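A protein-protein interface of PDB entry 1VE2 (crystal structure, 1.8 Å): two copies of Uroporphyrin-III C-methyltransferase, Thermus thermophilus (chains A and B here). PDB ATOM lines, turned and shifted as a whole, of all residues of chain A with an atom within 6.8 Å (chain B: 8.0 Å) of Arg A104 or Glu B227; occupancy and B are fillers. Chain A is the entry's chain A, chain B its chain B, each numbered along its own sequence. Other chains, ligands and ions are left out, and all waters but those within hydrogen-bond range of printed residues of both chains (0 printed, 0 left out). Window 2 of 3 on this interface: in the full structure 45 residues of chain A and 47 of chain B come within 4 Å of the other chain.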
ATOM      1  N   ILE A  72      15.558 -37.599 -29.158  1.00  0.00           N
ATOM      2  CA  ILE A  72      15.218 -36.711 -30.254  1.00  0.00           C
ATOM      3  C   ILE A  72      14.055 -37.291 -31.055  1.00  0.00           C
ATOM      4  O   ILE A  72      13.093 -36.585 -31.344  1.00  0.00           O
ATOM      5  CB  ILE A  72      16.440 -36.476 -31.177  1.00  0.00           C
ATOM      6  CG1 ILE A  72      17.509 -35.680 -30.413  1.00  0.00           C
ATOM      7  CG2 ILE A  72      16.021 -35.728 -32.450  1.00  0.00           C
ATOM      8  CD1 ILE A  72      18.848 -35.569 -31.126  1.00  0.00           C
ATOM      9  N   ARG A  76      10.269 -35.531 -31.544  1.00  0.00           N
ATOM     10  CA  ARG A  76       9.781 -35.176 -32.869  1.00  0.00           C
ATOM     11  C   ARG A  76       8.444 -35.855 -33.157  1.00  0.00           C
ATOM     12  O   ARG A  76       7.679 -35.398 -34.006  1.00  0.00           O
ATOM     13  CB  ARG A  76      10.836 -35.523 -33.923  1.00  0.00           C
ATOM     14  CG  ARG A  76      11.990 -34.519 -33.924  1.00  0.00           C
ATOM     15  CD  ARG A  76      13.119 -34.900 -34.866  1.00  0.00           C
ATOM     16  NE  ARG A  76      14.060 -33.792 -35.024  1.00  0.00           N
ATOM     17  CZ  ARG A  76      15.291 -33.916 -35.511  1.00  0.00           C
ATOM     18  NH1 ARG A  76      15.742 -35.106 -35.892  1.00  0.00           N
ATOM     19  NH2 ARG A  76      16.071 -32.849 -35.620  1.00  0.00           N
ATOM     20  N   GLU A  97      26.553 -33.515 -23.185  1.00  0.00           N
ATOM     21  CA  GLU A  97      26.487 -33.895 -24.587  1.00  0.00           C
ATOM     22  C   GLU A  97      25.033 -34.073 -25.025  1.00  0.00           C
ATOM     23  O   GLU A  97      24.679 -33.756 -26.165  1.00  0.00           O
ATOM     24  CB  GLU A  97      27.271 -35.183 -24.823  1.00  0.00           C
ATOM     25  CG  GLU A  97      28.762 -35.013 -24.672  1.00  0.00           C
ATOM     26  CD  GLU A  97      29.487 -36.291 -24.985  1.00  0.00           C
ATOM     27  OE1 GLU A  97      30.306 -36.723 -24.158  1.00  0.00           O
ATOM     28  OE2 GLU A  97      29.224 -36.865 -26.059  1.00  0.00           O
ATOM     29  N   ALA A  99      22.431 -32.462 -23.748  1.00  0.00           N
ATOM     30  CA  ALA A  99      21.885 -31.108 -23.864  1.00  0.00           C
ATOM     31  C   ALA A  99      22.312 -30.471 -25.185  1.00  0.00           C
ATOM     32  O   ALA A  99      21.496 -29.880 -25.882  1.00  0.00           O
ATOM     33  CB  ALA A  99      22.366 -30.245 -22.704  1.00  0.00           C
ATOM     34  N   LEU A 100      23.598 -30.567 -25.517  1.00  0.00           N
ATOM     35  CA  LEU A 100      24.095 -29.994 -26.770  1.00  0.00           C
ATOM     36  C   LEU A 100      23.392 -30.598 -27.979  1.00  0.00           C
ATOM     37  O   LEU A 100      23.013 -29.889 -28.912  1.00  0.00           O
ATOM     38  CB  LEU A 100      25.598 -30.232 -26.919  1.00  0.00           C
ATOM     39  CG  LEU A 100      26.557 -29.156 -26.437  1.00  0.00           C
ATOM     40  CD1 LEU A 100      27.989 -29.637 -26.682  1.00  0.00           C
ATOM     41  CD2 LEU A 100      26.289 -27.842 -27.193  1.00  0.00           C
ATOM     42  N   ALA A 101      23.235 -31.919 -27.967  1.00  0.00           N
ATOM     43  CA  ALA A 101      22.581 -32.599 -29.076  1.00  0.00           C
ATOM     44  C   ALA A 101      21.142 -32.132 -29.247  1.00  0.00           C
ATOM     45  O   ALA A 101      20.677 -31.932 -30.371  1.00  0.00           O
ATOM     46  CB  ALA A 101      22.627 -34.112 -28.867  1.00  0.00           C
ATOM     47  N   LEU A 102      20.438 -31.939 -28.138  1.00  0.00           N
ATOM     48  CA  LEU A 102      19.047 -31.505 -28.220  1.00  0.00           C
ATOM     49  C   LEU A 102      18.975 -30.097 -28.791  1.00  0.00           C
ATOM     50  O   LEU A 102      18.139 -29.812 -29.655  1.00  0.00           O
ATOM     51  CB  LEU A 102      18.390 -31.563 -26.836  1.00  0.00           C
ATOM     52  CG  LEU A 102      18.263 -32.977 -26.251  1.00  0.00           C
ATOM     53  CD1 LEU A 102      17.847 -32.896 -24.794  1.00  0.00           C
ATOM     54  CD2 LEU A 102      17.258 -33.786 -27.056  1.00  0.00           C
ATOM     55  N   ARG A 103      19.854 -29.220 -28.313  1.00  0.00           N
ATOM     56  CA  ARG A 103      19.904 -27.846 -28.796  1.00  0.00           C
ATOM     57  C   ARG A 103      20.166 -27.844 -30.299  1.00  0.00           C
ATOM     58  O   ARG A 103      19.457 -27.198 -31.065  1.00  0.00           O
ATOM     59  CB  ARG A 103      21.029 -27.070 -28.091  1.00  0.00           C
ATOM     60  CG  ARG A 103      21.154 -25.612 -28.510  1.00  0.00           C
ATOM     61  CD  ARG A 103      20.547 -24.659 -27.469  1.00  0.00           C
ATOM     62  NE  ARG A 103      19.120 -24.875 -27.275  1.00  0.00           N
ATOM     63  CZ  ARG A 103      18.403 -24.351 -26.284  1.00  0.00           C
ATOM     64  NH1 ARG A 103      18.976 -23.571 -25.377  1.00  0.00           N
ATOM     65  NH2 ARG A 103      17.104 -24.607 -26.198  1.00  0.00           N
ATOM     66  N   ARG A 104      21.193 -28.577 -30.718  1.00  0.00           N
ATOM     67  CA  ARG A 104      21.548 -28.636 -32.130  1.00  0.00           C
ATOM     68  C   ARG A 104      20.476 -29.287 -32.996  1.00  0.00           C
ATOM     69  O   ARG A 104      20.413 -29.030 -34.196  1.00  0.00           O
ATOM     70  CB  ARG A 104      22.893 -29.352 -32.296  1.00  0.00           C
ATOM     71  CG  ARG A 104      24.052 -28.514 -31.767  1.00  0.00           C
ATOM     72  CD  ARG A 104      25.357 -29.293 -31.580  1.00  0.00           C
ATOM     73  NE  ARG A 104      26.410 -28.401 -31.090  1.00  0.00           N
ATOM     74  CZ  ARG A 104      27.634 -28.792 -30.730  1.00  0.00           C
ATOM     75  NH1 ARG A 104      27.975 -30.069 -30.802  1.00  0.00           N
ATOM     76  NH2 ARG A 104      28.520 -27.899 -30.302  1.00  0.00           N
ATOM     77  N   ALA A 105      19.630 -30.119 -32.398  1.00  0.00           N
ATOM     78  CA  ALA A 105      18.565 -30.767 -33.162  1.00  0.00           C
ATOM     79  C   ALA A 105      17.297 -29.917 -33.167  1.00  0.00           C
ATOM     80  O   ALA A 105      16.319 -30.252 -33.841  1.00  0.00           O
ATOM     81  CB  ALA A 105      18.272 -32.155 -32.591  1.00  0.00           C
ATOM     82  N   GLY A 106      17.315 -28.823 -32.415  1.00  0.00           N
ATOM     83  CA  GLY A 106      16.160 -27.943 -32.336  1.00  0.00           C
ATOM     84  C   GLY A 106      15.026 -28.517 -31.502  1.00  0.00           C
ATOM     85  O   GLY A 106      13.859 -28.202 -31.730  1.00  0.00           O
ATOM     86  N   ILE A 107      15.368 -29.359 -30.527  1.00  0.00           N
ATOM     87  CA  ILE A 107      14.375 -29.991 -29.660  1.00  0.00           C
ATOM     88  C   ILE A 107      14.218 -29.238 -28.343  1.00  0.00           C
ATOM     89  O   ILE A 107      15.200 -28.991 -27.642  1.00  0.00           O
ATOM     90  CB  ILE A 107      14.780 -31.448 -29.321  1.00  0.00           C
ATOM     91  CG1 ILE A 107      14.968 -32.254 -30.606  1.00  0.00           C
ATOM     92  CG2 ILE A 107      13.730 -32.094 -28.433  1.00  0.00           C
ATOM     93  CD1 ILE A 107      13.740 -32.289 -31.498  1.00  0.00           C
ATOM     94  N   PHE A 109      13.990 -28.515 -24.610  1.00  0.00           N
ATOM     95  CA  PHE A 109      14.411 -29.324 -23.467  1.00  0.00           C
ATOM     96  C   PHE A 109      14.645 -28.482 -22.222  1.00  0.00           C
ATOM     97  O   PHE A 109      14.868 -27.273 -22.308  1.00  0.00           O
ATOM     98  CB  PHE A 109      15.687 -30.111 -23.807  1.00  0.00           C
ATOM     99  CG  PHE A 109      16.935 -29.274 -23.825  1.00  0.00           C
ATOM    100  CD1 PHE A 109      17.720 -29.148 -22.678  1.00  0.00           C
ATOM    101  CD2 PHE A 109      17.311 -28.588 -24.976  1.00  0.00           C
ATOM    102  CE1 PHE A 109      18.870 -28.342 -22.679  1.00  0.00           C
ATOM    103  CE2 PHE A 109      18.457 -27.780 -24.987  1.00  0.00           C
ATOM    104  CZ  PHE A 109      19.236 -27.661 -23.831  1.00  0.00           C
ATOM    105  N   GLY B 126      20.936 -25.654 -17.745  1.00  0.00           N
ATOM    106  CA  GLY B 126      21.355 -26.569 -18.799  1.00  0.00           C
ATOM    107  C   GLY B 126      22.848 -26.469 -19.080  1.00  0.00           C
ATOM    108  O   GLY B 126      23.313 -26.796 -20.182  1.00  0.00           O
ATOM    109  N   LEU B 127      23.605 -26.040 -18.074  1.00  0.00           N
ATOM    110  CA  LEU B 127      25.053 -25.856 -18.219  1.00  0.00           C
ATOM    111  C   LEU B 127      25.837 -26.880 -17.409  1.00  0.00           C
ATOM    112  O   LEU B 127      25.662 -26.989 -16.197  1.00  0.00           O
ATOM    113  CB  LEU B 127      25.434 -24.439 -17.774  1.00  0.00           C
ATOM    114  CG  LEU B 127      24.622 -23.313 -18.440  1.00  0.00           C
ATOM    115  CD1 LEU B 127      25.054 -21.986 -17.817  1.00  0.00           C
ATOM    116  CD2 LEU B 127      24.818 -23.302 -19.950  1.00  0.00           C
ATOM    117  N   HIS B 131      32.501 -32.516 -19.292  1.00  0.00           N
ATOM    118  CA  HIS B 131      32.268 -32.935 -20.679  1.00  0.00           C
ATOM    119  C   HIS B 131      33.492 -33.793 -21.045  1.00  0.00           C
ATOM    120  O   HIS B 131      34.628 -33.359 -20.880  1.00  0.00           O
ATOM    121  CB  HIS B 131      32.161 -31.704 -21.591  1.00  0.00           C
ATOM    122  CG  HIS B 131      31.899 -32.026 -23.033  1.00  0.00           C
ATOM    123  ND1 HIS B 131      32.866 -32.544 -23.870  1.00  0.00           N
ATOM    124  CD2 HIS B 131      30.789 -31.868 -23.794  1.00  0.00           C
ATOM    125  CE1 HIS B 131      32.364 -32.684 -25.085  1.00  0.00           C
ATOM    126  NE2 HIS B 131      31.106 -32.281 -25.067  1.00  0.00           N
ATOM    127  N   LEU B 197      28.859 -13.882 -20.184  1.00  0.00           N
ATOM    128  CA  LEU B 197      29.790 -14.850 -20.766  1.00  0.00           C
ATOM    129  C   LEU B 197      30.973 -14.092 -21.370  1.00  0.00           C
ATOM    130  O   LEU B 197      30.798 -13.111 -22.105  1.00  0.00           O
ATOM    131  CB  LEU B 197      29.099 -15.663 -21.863  1.00  0.00           C
ATOM    132  CG  LEU B 197      27.886 -16.505 -21.457  1.00  0.00           C
ATOM    133  CD1 LEU B 197      27.335 -17.208 -22.695  1.00  0.00           C
ATOM    134  CD2 LEU B 197      28.282 -17.527 -20.384  1.00  0.00           C
ATOM    135  N   VAL B 222      33.155 -24.010 -20.342  1.00  0.00           N
ATOM    136  CA  VAL B 222      32.365 -22.780 -20.377  1.00  0.00           C
ATOM    137  C   VAL B 222      32.200 -22.269 -21.811  1.00  0.00           C
ATOM    138  O   VAL B 222      31.295 -21.478 -22.108  1.00  0.00           O
ATOM    139  CB  VAL B 222      33.012 -21.705 -19.461  1.00  0.00           C
ATOM    140  CG1 VAL B 222      32.251 -20.386 -19.573  1.00  0.00           C
ATOM    141  CG2 VAL B 222      32.979 -22.194 -17.997  1.00  0.00           C
ATOM    142  N   GLY B 223      33.063 -22.731 -22.710  1.00  0.00           N
ATOM    143  CA  GLY B 223      32.951 -22.313 -24.099  1.00  0.00           C
ATOM    144  C   GLY B 223      31.654 -22.795 -24.732  1.00  0.00           C
ATOM    145  O   GLY B 223      31.248 -22.309 -25.784  1.00  0.00           O
ATOM    146  N   LEU B 224      30.997 -23.765 -24.102  1.00  0.00           N
ATOM    147  CA  LEU B 224      29.745 -24.314 -24.625  1.00  0.00           C
ATOM    148  C   LEU B 224      28.500 -23.541 -24.190  1.00  0.00           C
ATOM    149  O   LEU B 224      27.429 -23.695 -24.778  1.00  0.00           O
ATOM    150  CB  LEU B 224      29.577 -25.751 -24.127  1.00  0.00           C
ATOM    151  CG  LEU B 224      29.962 -27.007 -24.910  1.00  0.00           C
ATOM    152  CD1 LEU B 224      31.082 -26.776 -25.882  1.00  0.00           C
ATOM    153  CD2 LEU B 224      30.278 -28.088 -23.889  1.00  0.00           C
ATOM    154  N   TYR B 225      28.645 -22.715 -23.163  1.00  0.00           N
ATOM    155  CA  TYR B 225      27.504 -22.005 -22.591  1.00  0.00           C
ATOM    156  C   TYR B 225      26.706 -21.098 -23.519  1.00  0.00           C
ATOM    157  O   TYR B 225      25.479 -21.023 -23.409  1.00  0.00           O
ATOM    158  CB  TYR B 225      27.963 -21.230 -21.358  1.00  0.00           C
ATOM    159  CG  TYR B 225      28.403 -22.118 -20.204  1.00  0.00           C
ATOM    160  CD1 TYR B 225      28.627 -23.490 -20.385  1.00  0.00           C
ATOM    161  CD2 TYR B 225      28.624 -21.577 -18.938  1.00  0.00           C
ATOM    162  CE1 TYR B 225      29.057 -24.296 -19.326  1.00  0.00           C
ATOM    163  CE2 TYR B 225      29.057 -22.373 -17.872  1.00  0.00           C
ATOM    164  CZ  TYR B 225      29.270 -23.729 -18.071  1.00  0.00           C
ATOM    165  OH  TYR B 225      29.684 -24.508 -17.011  1.00  0.00           O
ATOM    166  N   GLY B 226      27.396 -20.405 -24.416  1.00  0.00           N
ATOM    167  CA  GLY B 226      26.706 -19.531 -25.352  1.00  0.00           C
ATOM    168  C   GLY B 226      25.745 -20.321 -26.221  1.00  0.00           C
ATOM    169  O   GLY B 226      24.619 -19.892 -26.473  1.00  0.00           O
ATOM    170  N   GLU B 227      26.176 -21.485 -26.687  1.00  0.00           N
ATOM    171  CA  GLU B 227      25.303 -22.299 -27.520  1.00  0.00           C
ATOM    172  C   GLU B 227      24.191 -22.983 -26.714  1.00  0.00           C
ATOM    173  O   GLU B 227      23.070 -23.129 -27.204  1.00  0.00           O
ATOM    174  CB  GLU B 227      26.121 -23.353 -28.277  1.00  0.00           C
ATOM    175  CG  GLU B 227      25.282 -24.226 -29.218  1.00  0.00           C
ATOM    176  CD  GLU B 227      26.133 -25.126 -30.098  1.00  0.00           C
ATOM    177  OE1 GLU B 227      27.356 -25.216 -29.849  1.00  0.00           O
ATOM    178  OE2 GLU B 227      25.579 -25.752 -31.034  1.00  0.00           O
ATOM    179  N   LEU B 228      24.500 -23.390 -25.482  1.00  0.00           N
ATOM    180  CA  LEU B 228      23.528 -24.084 -24.633  1.00  0.00           C
ATOM    181  C   LEU B 228      22.407 -23.202 -24.091  1.00  0.00           C
ATOM    182  O   LEU B 228      21.284 -23.664 -23.902  1.00  0.00           O
ATOM    183  CB  LEU B 228      24.246 -24.774 -23.467  1.00  0.00           C
ATOM    184  CG  LEU B 228      25.023 -26.044 -23.828  1.00  0.00           C
ATOM    185  CD1 LEU B 228      25.929 -26.429 -22.683  1.00  0.00           C
ATOM    186  CD2 LEU B 228      24.051 -27.178 -24.145  1.00  0.00           C
ATOM    187  N   LEU B 229      22.713 -21.937 -23.836  1.00  0.00           N
ATOM    188  CA  LEU B 229      21.713 -21.008 -23.325  1.00  0.00           C
ATOM    189  C   LEU B 229      20.761 -20.537 -24.425  1.00  0.00           C
ATOM    190  O   LEU B 229      21.117 -20.500 -25.603  1.00  0.00           O
ATOM    191  CB  LEU B 229      22.398 -19.787 -22.698  1.00  0.00           C
ATOM    192  CG  LEU B 229      23.100 -20.027 -21.359  1.00  0.00           C
ATOM    193  CD1 LEU B 229      23.916 -18.806 -20.949  1.00  0.00           C
ATOM    194  CD2 LEU B 229      22.051 -20.357 -20.312  1.00  0.00           C
ATOM    195  N   PRO B 230      19.523 -20.189 -24.047  1.00  0.00           N
ATOM    196  CA  PRO B 230      18.544 -19.713 -25.029  1.00  0.00           C
ATOM    197  C   PRO B 230      19.041 -18.378 -25.591  1.00  0.00           C
ATOM    198  O   PRO B 230      19.795 -17.663 -24.924  1.00  0.00           O
ATOM    199  CB  PRO B 230      17.275 -19.552 -24.196  1.00  0.00           C
ATOM    200  CG  PRO B 230      17.432 -20.607 -23.133  1.00  0.00           C
ATOM    201  CD  PRO B 230      18.883 -20.443 -22.743  1.00  0.00           C
ATOM    202  N   LYS B 231      18.637 -18.046 -26.811  1.00  0.00           N
ATOM    203  CA  LYS B 231      19.053 -16.785 -27.428  1.00  0.00           C
ATOM    204  C   LYS B 231      18.642 -15.577 -26.582  1.00  0.00           C
ATOM    205  O   LYS B 231      17.541 -15.034 -26.825  1.00  0.00           O
ATOM    206  CB  LYS B 231      18.451 -16.649 -28.826  1.00  0.00           C
ATOM    207  CG  LYS B 231      19.002 -17.620 -29.848  1.00  0.00           C
ATOM    208  CD  LYS B 231      18.342 -17.385 -31.196  1.00  0.00           C
ATOM    209  CE  LYS B 231      18.883 -18.325 -32.264  1.00  0.00           C
ATOM    210  NZ  LYS B 231      18.237 -18.062 -33.580  1.00  0.00           N
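O of Leu B228 lies within hydrogen-bond range of NH1 of Arg A103 (2.7 Å). The guanidinium group (NE) of Arg A104 lies within salt-bridge range of the side-chain carboxylate (OE2) of Glu B227, 2.8 Å away.
Of chain B, only Glu B227 comes within 4 Å of Arg A104. Of chain A, only Leu A100 (3.9 Å), Arg A103 (3.0 Å) and Arg A104 (2.8 Å) come within 4 Å of Glu B227. Of the printed residues of chain A, Leu B224 touches Leu A100. Of the printed residues of chain A, Leu B228 touches Ala A99, Leu A100 and Arg A103. Of the printed residues of chain B, Glu A97 touches His B131 (3.6 Å). Of the printed residues of chain A, Pro B230 touches Arg A103. Printed residues of chain B within 4 Å of Ala A99: Leu B228 (3.8 Å). Gly B223 touches none of the printed residues of chain A. Arg A76 touches none of the printed residues of chain B. The nearest printed residue of chain A that does not touch Glu B227 is Phe A109 (6.8 Å). The nearest printed residue of chain B that does not touch Arg A103 is Lys B231 (5.7 Å).
Of the 13 printed residues of chain A, 5 touch a printed residue of chain B. Hydrophobic or aromatic side chains of chain A within 4 Å of the printed part of chain B: Ala A99 and Leu A100. Among the printed residues, 10 pairs touch across the chains.
Among the printed residues, pairs that only touch across the chains: Arg A103 with Glu B227 (3.0 Å), Glu A97 with His B131 (3.6 Å), Arg A103 with Leu B229 (3.6 Å), Arg A103 with Pro B230 (3.7 Å), Leu A100 with Leu B228 (3.7 Å), Leu A100 with Leu B224 (3.7 Å), Ala A99 with Leu B228 (3.8 Å) and Leu A100 with Glu B227 (3.9 Å).
No position is printed for both chains. Of the 10 pairs that touch across the chains among the printed residues, none has its exchanged pair printed and touching as well.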
